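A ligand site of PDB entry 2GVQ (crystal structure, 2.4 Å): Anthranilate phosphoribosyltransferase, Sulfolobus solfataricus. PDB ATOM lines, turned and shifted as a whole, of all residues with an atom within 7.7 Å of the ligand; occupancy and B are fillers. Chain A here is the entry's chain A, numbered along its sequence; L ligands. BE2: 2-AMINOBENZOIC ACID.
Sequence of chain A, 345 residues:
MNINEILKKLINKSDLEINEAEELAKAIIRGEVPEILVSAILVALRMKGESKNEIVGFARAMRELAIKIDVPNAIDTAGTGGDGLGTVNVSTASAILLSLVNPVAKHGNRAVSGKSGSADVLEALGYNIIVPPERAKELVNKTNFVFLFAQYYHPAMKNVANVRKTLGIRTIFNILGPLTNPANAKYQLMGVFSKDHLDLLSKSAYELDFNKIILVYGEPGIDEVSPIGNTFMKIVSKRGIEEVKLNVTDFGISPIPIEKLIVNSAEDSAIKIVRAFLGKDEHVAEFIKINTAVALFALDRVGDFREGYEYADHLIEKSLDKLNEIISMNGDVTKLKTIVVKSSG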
ATOM      1  N   MET A  62     -31.547  22.793 -19.622  1.00  0.00           N
ATOM      2  CA  MET A  62     -31.777  22.631 -18.190  1.00  0.00           C
ATOM      3  C   MET A  62     -31.975  23.982 -17.536  1.00  0.00           C
ATOM      4  O   MET A  62     -32.749  24.109 -16.585  1.00  0.00           O
ATOM      5  CB  MET A  62     -30.611  21.908 -17.518  1.00  0.00           C
ATOM      6  CG  MET A  62     -30.569  20.423 -17.787  1.00  0.00           C
ATOM      7  SD  MET A  62     -29.509  19.574 -16.595  1.00  0.00           S
ATOM      8  CE  MET A  62     -27.960  20.134 -17.116  1.00  0.00           C
ATOM      9  N   HIS A 107     -24.149  25.867  -5.910  1.00  0.00           N
ATOM     10  CA  HIS A 107     -25.040  24.881  -6.525  1.00  0.00           C
ATOM     11  C   HIS A 107     -24.409  23.501  -6.311  1.00  0.00           C
ATOM     12  O   HIS A 107     -23.215  23.358  -6.536  1.00  0.00           O
ATOM     13  CB  HIS A 107     -25.164  25.183  -8.025  1.00  0.00           C
ATOM     14  CG  HIS A 107     -26.092  24.274  -8.773  1.00  0.00           C
ATOM     15  ND1 HIS A 107     -25.932  23.981 -10.106  1.00  0.00           N
ATOM     16  CD2 HIS A 107     -27.216  23.624  -8.374  1.00  0.00           C
ATOM     17  CE1 HIS A 107     -26.907  23.189 -10.513  1.00  0.00           C
ATOM     18  NE2 HIS A 107     -27.703  22.957  -9.478  1.00  0.00           N
ATOM     19  N   GLY A 108     -25.193  22.511  -5.891  1.00  0.00           N
ATOM     20  CA  GLY A 108     -24.629  21.176  -5.692  1.00  0.00           C
ATOM     21  C   GLY A 108     -25.630  20.116  -5.280  1.00  0.00           C
ATOM     22  O   GLY A 108     -26.803  20.406  -5.085  1.00  0.00           O
ATOM     23  N   ASN A 109     -25.165  18.871  -5.142  1.00  0.00           N
ATOM     24  CA  ASN A 109     -26.003  17.731  -4.747  1.00  0.00           C
ATOM     25  C   ASN A 109     -25.277  16.966  -3.638  1.00  0.00           C
ATOM     26  O   ASN A 109     -24.190  17.363  -3.201  1.00  0.00           O
ATOM     27  CB  ASN A 109     -26.184  16.738  -5.914  1.00  0.00           C
ATOM     28  CG  ASN A 109     -27.547  16.838  -6.580  1.00  0.00           C
ATOM     29  OD1 ASN A 109     -28.549  17.076  -5.914  1.00  0.00           O
ATOM     30  ND2 ASN A 109     -27.582  16.631  -7.896  1.00  0.00           N
ATOM     31  N   PHE A 149     -29.685  23.398  -3.712  1.00  0.00           N
ATOM     32  CA  PHE A 149     -29.721  21.937  -3.839  1.00  0.00           C
ATOM     33  C   PHE A 149     -30.302  21.539  -5.214  1.00  0.00           C
ATOM     34  O   PHE A 149     -31.516  21.474  -5.394  1.00  0.00           O
ATOM     35  CB  PHE A 149     -30.593  21.380  -2.689  1.00  0.00           C
ATOM     36  CG  PHE A 149     -30.340  19.933  -2.354  1.00  0.00           C
ATOM     37  CD1 PHE A 149     -30.928  19.351  -1.233  1.00  0.00           C
ATOM     38  CD2 PHE A 149     -29.540  19.137  -3.158  1.00  0.00           C
ATOM     39  CE1 PHE A 149     -30.723  17.995  -0.920  1.00  0.00           C
ATOM     40  CE2 PHE A 149     -29.340  17.784  -2.864  1.00  0.00           C
ATOM     41  CZ  PHE A 149     -29.921  17.214  -1.742  1.00  0.00           C
ATOM     42  N   ALA A 150     -29.410  21.293  -6.189  1.00  0.00           N
ATOM     43  CA  ALA A 150     -29.766  20.909  -7.579  1.00  0.00           C
ATOM     44  C   ALA A 150     -30.949  19.953  -7.730  1.00  0.00           C
ATOM     45  O   ALA A 150     -31.824  20.135  -8.575  1.00  0.00           O
ATOM     46  CB  ALA A 150     -28.530  20.290  -8.266  1.00  0.00           C
ATOM     47  N   GLN A 151     -30.959  18.906  -6.919  1.00  0.00           N
ATOM     48  CA  GLN A 151     -32.013  17.914  -6.953  1.00  0.00           C
ATOM     49  C   GLN A 151     -33.419  18.545  -6.872  1.00  0.00           C
ATOM     50  O   GLN A 151     -34.369  18.001  -7.416  1.00  0.00           O
ATOM     51  CB  GLN A 151     -31.798  16.967  -5.783  1.00  0.00           C
ATOM     52  CG  GLN A 151     -32.698  15.781  -5.760  1.00  0.00           C
ATOM     53  CD  GLN A 151     -32.343  14.895  -4.606  1.00  0.00           C
ATOM     54  OE1 GLN A 151     -31.177  14.860  -4.180  1.00  0.00           O
ATOM     55  NE2 GLN A 151     -33.315  14.144  -4.109  1.00  0.00           N
ATOM     56  N   TYR A 152     -33.526  19.684  -6.178  1.00  0.00           N
ATOM     57  CA  TYR A 152     -34.793  20.391  -6.004  1.00  0.00           C
ATOM     58  C   TYR A 152     -34.933  21.589  -6.945  1.00  0.00           C
ATOM     59  O   TYR A 152     -36.052  21.947  -7.331  1.00  0.00           O
ATOM     60  CB  TYR A 152     -34.947  20.862  -4.542  1.00  0.00           C
ATOM     61  CG  TYR A 152     -35.130  19.707  -3.589  1.00  0.00           C
ATOM     62  CD1 TYR A 152     -36.309  18.957  -3.595  1.00  0.00           C
ATOM     63  CD2 TYR A 152     -34.074  19.247  -2.795  1.00  0.00           C
ATOM     64  CE1 TYR A 152     -36.437  17.794  -2.870  1.00  0.00           C
ATOM     65  CE2 TYR A 152     -34.180  18.061  -2.048  1.00  0.00           C
ATOM     66  CZ  TYR A 152     -35.376  17.340  -2.097  1.00  0.00           C
ATOM     67  OH  TYR A 152     -35.512  16.125  -1.464  1.00  0.00           O
ATOM     68  N   TYR A 153     -33.817  22.209  -7.316  1.00  0.00           N
ATOM     69  CA  TYR A 153     -33.863  23.345  -8.231  1.00  0.00           C
ATOM     70  C   TYR A 153     -33.871  22.895  -9.687  1.00  0.00           C
ATOM     71  O   TYR A 153     -33.822  23.724 -10.604  1.00  0.00           O
ATOM     72  CB  TYR A 153     -32.679  24.281  -7.958  1.00  0.00           C
ATOM     73  CG  TYR A 153     -32.912  25.182  -6.771  1.00  0.00           C
ATOM     74  CD1 TYR A 153     -32.699  24.724  -5.463  1.00  0.00           C
ATOM     75  CD2 TYR A 153     -33.400  26.484  -6.945  1.00  0.00           C
ATOM     76  CE1 TYR A 153     -32.962  25.535  -4.360  1.00  0.00           C
ATOM     77  CE2 TYR A 153     -33.666  27.306  -5.848  1.00  0.00           C
ATOM     78  CZ  TYR A 153     -33.445  26.835  -4.566  1.00  0.00           C
ATOM     79  OH  TYR A 153     -33.717  27.661  -3.488  1.00  0.00           O
ATOM     80  N   HIS A 154     -33.919  21.578  -9.899  1.00  0.00           N
ATOM     81  CA  HIS A 154     -33.963  20.972 -11.217  1.00  0.00           C
ATOM     82  C   HIS A 154     -34.941  19.802 -11.148  1.00  0.00           C
ATOM     83  O   HIS A 154     -34.588  18.663 -11.444  1.00  0.00           O
ATOM     84  CB  HIS A 154     -32.595  20.456 -11.624  1.00  0.00           C
ATOM     85  CG  HIS A 154     -31.612  21.534 -11.912  1.00  0.00           C
ATOM     86  ND1 HIS A 154     -31.628  22.249 -13.097  1.00  0.00           N
ATOM     87  CD2 HIS A 154     -30.604  22.053 -11.178  1.00  0.00           C
ATOM     88  CE1 HIS A 154     -30.670  23.160 -13.063  1.00  0.00           C
ATOM     89  NE2 HIS A 154     -30.041  23.066 -11.902  1.00  0.00           N
ATOM     90  N   PRO A 155     -36.194  20.081 -10.755  1.00  0.00           N
ATOM     91  CA  PRO A 155     -37.189  19.007 -10.663  1.00  0.00           C
ATOM     92  C   PRO A 155     -37.421  18.201 -11.948  1.00  0.00           C
ATOM     93  O   PRO A 155     -37.723  17.004 -11.899  1.00  0.00           O
ATOM     94  CB  PRO A 155     -38.427  19.756 -10.172  1.00  0.00           C
ATOM     95  CG  PRO A 155     -38.288  21.080 -10.816  1.00  0.00           C
ATOM     96  CD  PRO A 155     -36.820  21.400 -10.592  1.00  0.00           C
ATOM     97  N   ALA A 156     -37.263  18.836 -13.101  1.00  0.00           N
ATOM     98  CA  ALA A 156     -37.471  18.158 -14.378  1.00  0.00           C
ATOM     99  C   ALA A 156     -36.556  16.946 -14.546  1.00  0.00           C
ATOM    100  O   ALA A 156     -36.838  16.038 -15.321  1.00  0.00           O
ATOM    101  CB  ALA A 156     -37.261  19.148 -15.528  1.00  0.00           C
ATOM    102  N   MET A 157     -35.453  16.939 -13.812  1.00  0.00           N
ATOM    103  CA  MET A 157     -34.508  15.833 -13.925  1.00  0.00           C
ATOM    104  C   MET A 157     -35.084  14.479 -13.526  1.00  0.00           C
ATOM    105  O   MET A 157     -34.507  13.439 -13.843  1.00  0.00           O
ATOM    106  CB  MET A 157     -33.257  16.166 -13.102  1.00  0.00           C
ATOM    107  CG  MET A 157     -32.418  17.243 -13.752  1.00  0.00           C
ATOM    108  SD  MET A 157     -32.066  16.799 -15.473  1.00  0.00           S
ATOM    109  CE  MET A 157     -30.947  15.394 -15.174  1.00  0.00           C
ATOM    110  N   LYS A 158     -36.222  14.493 -12.858  1.00  0.00           N
ATOM    111  CA  LYS A 158     -36.874  13.247 -12.449  1.00  0.00           C
ATOM    112  C   LYS A 158     -37.262  12.442 -13.681  1.00  0.00           C
ATOM    113  O   LYS A 158     -37.377  11.214 -13.626  1.00  0.00           O
ATOM    114  CB  LYS A 158     -38.131  13.539 -11.641  1.00  0.00           C
ATOM    115  CG  LYS A 158     -39.203  14.229 -12.450  1.00  0.00           C
ATOM    116  CD  LYS A 158     -40.506  14.358 -11.693  1.00  0.00           C
ATOM    117  CE  LYS A 158     -41.665  14.516 -12.655  1.00  0.00           C
ATOM    118  NZ  LYS A 158     -42.613  13.351 -12.541  1.00  0.00           N
ATOM    119  N   ALA A 161     -34.419  10.181 -14.396  1.00  0.00           N
ATOM    120  CA  ALA A 161     -33.881   9.446 -13.251  1.00  0.00           C
ATOM    121  C   ALA A 161     -33.823   7.933 -13.434  1.00  0.00           C
ATOM    122  O   ALA A 161     -32.763   7.330 -13.291  1.00  0.00           O
ATOM    123  CB  ALA A 161     -34.683   9.796 -11.995  1.00  0.00           C
ATOM    124  N   ARG A 164     -31.134   6.921 -15.993  1.00  0.00           N
ATOM    125  CA  ARG A 164     -29.760   7.028 -15.522  1.00  0.00           C
ATOM    126  C   ARG A 164     -29.456   5.975 -14.449  1.00  0.00           C
ATOM    127  O   ARG A 164     -28.355   5.456 -14.363  1.00  0.00           O
ATOM    128  CB  ARG A 164     -29.491   8.432 -14.984  1.00  0.00           C
ATOM    129  CG  ARG A 164     -29.577   9.487 -16.073  1.00  0.00           C
ATOM    130  CD  ARG A 164     -28.671  10.664 -15.752  1.00  0.00           C
ATOM    131  NE  ARG A 164     -29.195  11.460 -14.654  1.00  0.00           N
ATOM    132  CZ  ARG A 164     -28.441  12.117 -13.781  1.00  0.00           C
ATOM    133  NH1 ARG A 164     -27.119  12.065 -13.854  1.00  0.00           N
ATOM    134  NH2 ARG A 164     -29.023  12.836 -12.841  1.00  0.00           N
ATOM    135  N   ILE A 172     -24.017  12.382 -20.292  1.00  0.00           N
ATOM    136  CA  ILE A 172     -23.788  13.798 -20.479  1.00  0.00           C
ATOM    137  C   ILE A 172     -24.244  14.573 -19.246  1.00  0.00           C
ATOM    138  O   ILE A 172     -23.715  15.642 -18.938  1.00  0.00           O
ATOM    139  CB  ILE A 172     -24.544  14.281 -21.741  1.00  0.00           C
ATOM    140  CG1 ILE A 172     -24.132  15.708 -22.091  1.00  0.00           C
ATOM    141  CG2 ILE A 172     -26.046  14.178 -21.512  1.00  0.00           C
ATOM    142  CD1 ILE A 172     -24.702  16.206 -23.400  1.00  0.00           C
ATOM    143  N   PHE A 173     -25.209  14.017 -18.513  1.00  0.00           N
ATOM    144  CA  PHE A 173     -25.752  14.672 -17.322  1.00  0.00           C
ATOM    145  C   PHE A 173     -24.793  14.801 -16.144  1.00  0.00           C
ATOM    146  O   PHE A 173     -24.910  15.726 -15.352  1.00  0.00           O
ATOM    147  CB  PHE A 173     -27.025  13.959 -16.863  1.00  0.00           C
ATOM    148  CG  PHE A 173     -28.204  14.221 -17.758  1.00  0.00           C
ATOM    149  CD1 PHE A 173     -28.725  13.216 -18.571  1.00  0.00           C
ATOM    150  CD2 PHE A 173     -28.775  15.491 -17.820  1.00  0.00           C
ATOM    151  CE1 PHE A 173     -29.799  13.469 -19.433  1.00  0.00           C
ATOM    152  CE2 PHE A 173     -29.852  15.763 -18.677  1.00  0.00           C
ATOM    153  CZ  PHE A 173     -30.357  14.739 -19.488  1.00  0.00           C
ATOM    154  N   ASN A 174     -23.858  13.859 -16.032  1.00  0.00           N
ATOM    155  CA  ASN A 174     -22.877  13.891 -14.952  1.00  0.00           C
ATOM    156  C   ASN A 174     -21.906  15.066 -15.050  1.00  0.00           C
ATOM    157  O   ASN A 174     -21.125  15.299 -14.130  1.00  0.00           O
ATOM    158  CB  ASN A 174     -22.081  12.576 -14.918  1.00  0.00           C
ATOM    159  CG  ASN A 174     -22.961  11.380 -14.628  1.00  0.00           C
ATOM    160  OD1 ASN A 174     -23.362  11.140 -13.480  1.00  0.00           O
ATOM    161  ND2 ASN A 174     -23.293  10.618 -15.656  1.00  0.00           N
ATOM    162  N   ILE A 175     -21.953  15.817 -16.145  1.00  0.00           N
ATOM    163  CA  ILE A 175     -21.059  16.959 -16.291  1.00  0.00           C
ATOM    164  C   ILE A 175     -21.737  18.302 -16.521  1.00  0.00           C
ATOM    165  O   ILE A 175     -21.066  19.311 -16.675  1.00  0.00           O
ATOM    166  CB  ILE A 175     -20.042  16.746 -17.430  1.00  0.00           C
ATOM    167  CG1 ILE A 175     -20.779  16.592 -18.768  1.00  0.00           C
ATOM    168  CG2 ILE A 175     -19.178  15.525 -17.132  1.00  0.00           C
ATOM    169  CD1 ILE A 175     -19.846  16.290 -19.954  1.00  0.00           C
ATOM    170  N   LEU A 176     -23.064  18.308 -16.519  1.00  0.00           N
ATOM    171  CA  LEU A 176     -23.802  19.547 -16.753  1.00  0.00           C
ATOM    172  C   LEU A 176     -24.096  20.393 -15.518  1.00  0.00           C
ATOM    173  O   LEU A 176     -24.103  21.623 -15.593  1.00  0.00           O
ATOM    174  CB  LEU A 176     -25.119  19.246 -17.456  1.00  0.00           C
ATOM    175  CG  LEU A 176     -24.981  18.877 -18.925  1.00  0.00           C
ATOM    176  CD1 LEU A 176     -26.301  18.389 -19.464  1.00  0.00           C
ATOM    177  CD2 LEU A 176     -24.468  20.085 -19.714  1.00  0.00           C
ATOM    178  N   GLY A 177     -24.331  19.749 -14.388  1.00  0.00           N
ATOM    179  CA  GLY A 177     -24.638  20.460 -13.166  1.00  0.00           C
ATOM    180  C   GLY A 177     -23.926  21.782 -12.943  1.00  0.00           C
ATOM    181  O   GLY A 177     -24.587  22.819 -12.720  1.00  0.00           O
ATOM    182  N   PRO A 178     -22.597  21.801 -13.004  1.00  0.00           N
ATOM    183  CA  PRO A 178     -21.891  23.059 -12.781  1.00  0.00           C
ATOM    184  C   PRO A 178     -22.159  24.149 -13.804  1.00  0.00           C
ATOM    185  O   PRO A 178     -21.830  25.324 -13.569  1.00  0.00           O
ATOM    186  CB  PRO A 178     -20.414  22.633 -12.705  1.00  0.00           C
ATOM    187  CG  PRO A 178     -20.362  21.371 -13.492  1.00  0.00           C
ATOM    188  CD  PRO A 178     -21.652  20.671 -13.142  1.00  0.00           C
ATOM    189  N   LEU A 179     -22.768  23.789 -14.932  1.00  0.00           N
ATOM    190  CA  LEU A 179     -23.048  24.776 -15.971  1.00  0.00           C
ATOM    191  C   LEU A 179     -24.526  25.192 -15.922  1.00  0.00           C
ATOM    192  O   LEU A 179     -25.004  25.943 -16.785  1.00  0.00           O
ATOM    193  CB  LEU A 179     -22.715  24.203 -17.353  1.00  0.00           C
ATOM    194  CG  LEU A 179     -21.269  23.761 -17.619  1.00  0.00           C
ATOM    195  CD1 LEU A 179     -21.268  22.869 -18.848  1.00  0.00           C
ATOM    196  CD2 LEU A 179     -20.329  24.967 -17.819  1.00  0.00           C
ATOM    197  N   THR A 180     -25.240  24.737 -14.900  1.00  0.00           N
ATOM    198  CA  THR A 180     -26.657  25.054 -14.782  1.00  0.00           C
ATOM    199  C   THR A 180     -27.025  25.658 -13.426  1.00  0.00           C
ATOM    200  O   THR A 180     -28.013  25.263 -12.814  1.00  0.00           O
ATOM    201  CB  THR A 180     -27.498  23.791 -15.000  1.00  0.00           C
ATOM    202  OG1 THR A 180     -27.228  22.844 -13.961  1.00  0.00           O
ATOM    203  CG2 THR A 180     -27.140  23.149 -16.340  1.00  0.00           C
ATOM    204  N   PRO A 182     -28.743  27.631 -10.817  1.00  0.00           N
ATOM    205  CA  PRO A 182     -30.097  28.202 -10.708  1.00  0.00           C
ATOM    206  C   PRO A 182     -30.137  29.720 -10.486  1.00  0.00           C
ATOM    207  O   PRO A 182     -31.120  30.385 -10.829  1.00  0.00           O
ATOM    208  CB  PRO A 182     -30.715  27.444  -9.529  1.00  0.00           C
ATOM    209  CG  PRO A 182     -29.989  26.159  -9.543  1.00  0.00           C
ATOM    210  CD  PRO A 182     -28.557  26.579  -9.796  1.00  0.00           C
HETATM  211  C   BE2 L   1     -29.896  16.209 -10.314  1.00  0.00           C
HETATM  212  O   BE2 L   1     -29.699  14.988 -10.131  1.00  0.00           O
HETATM  213  OXT BE2 L   1     -30.874  16.830  -9.697  1.00  0.00           O
HETATM  214  C1  BE2 L   1     -29.059  17.031 -11.245  1.00  0.00           C
HETATM  215  CA  BE2 L   1     -27.959  16.459 -11.970  1.00  0.00           C
HETATM  216  C3  BE2 L   1     -27.183  17.269 -12.856  1.00  0.00           C
HETATM  217  N   BE2 L   1     -27.603  15.143 -11.880  1.00  0.00           N
HETATM  218  C4  BE2 L   1     -27.498  18.627 -13.001  1.00  0.00           C
HETATM  219  C5  BE2 L   1     -28.565  19.219 -12.292  1.00  0.00           C
HETATM  220  C6  BE2 L   1     -29.340  18.434 -11.423  1.00  0.00           C
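The guanidinium group (NH2) of Arg 164 lies within salt-bridge range of an oxygen (O) of the ligand. N of Gln 151 lies close to OXT of the ligand (3.5 Å). An oxygen (O) of the ligand sits close to the side-chain amide nitrogen of Asn 109 (3.5 Å).
The backbone NH of Gln 151 lies within hydrogen-bond range of the side-chain amide oxygen of Asn 109. O of Gly 177 is in hydrogen-bond range of OG1 of Thr 180, at 2.9 Å. A ring nitrogen (ND1) of His 107 is in hydrogen-bond range of the backbone carbonyl oxygen (O) of Gly 177 (3.2 Å). The backbone NH (N) of Ala 150 sits at hydrogen-bond distance from the backbone carbonyl oxygen (O) of Gly 108 (3.0 Å). A ring nitrogen (NE2) of His 154 is in hydrogen-bond range of the backbone carbonyl oxygen of Thr 180, at 3.1 Å. NE2 of His 154 sits at hydrogen-bond distance from NE2 of His 107 (3.4 Å).
Residues that only touch the ligand: Gly 177, Ala 150, His 154 and Phe 173. Hydrophobic or aromatic side chains that line the ligand: Ala 150 and His 154.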
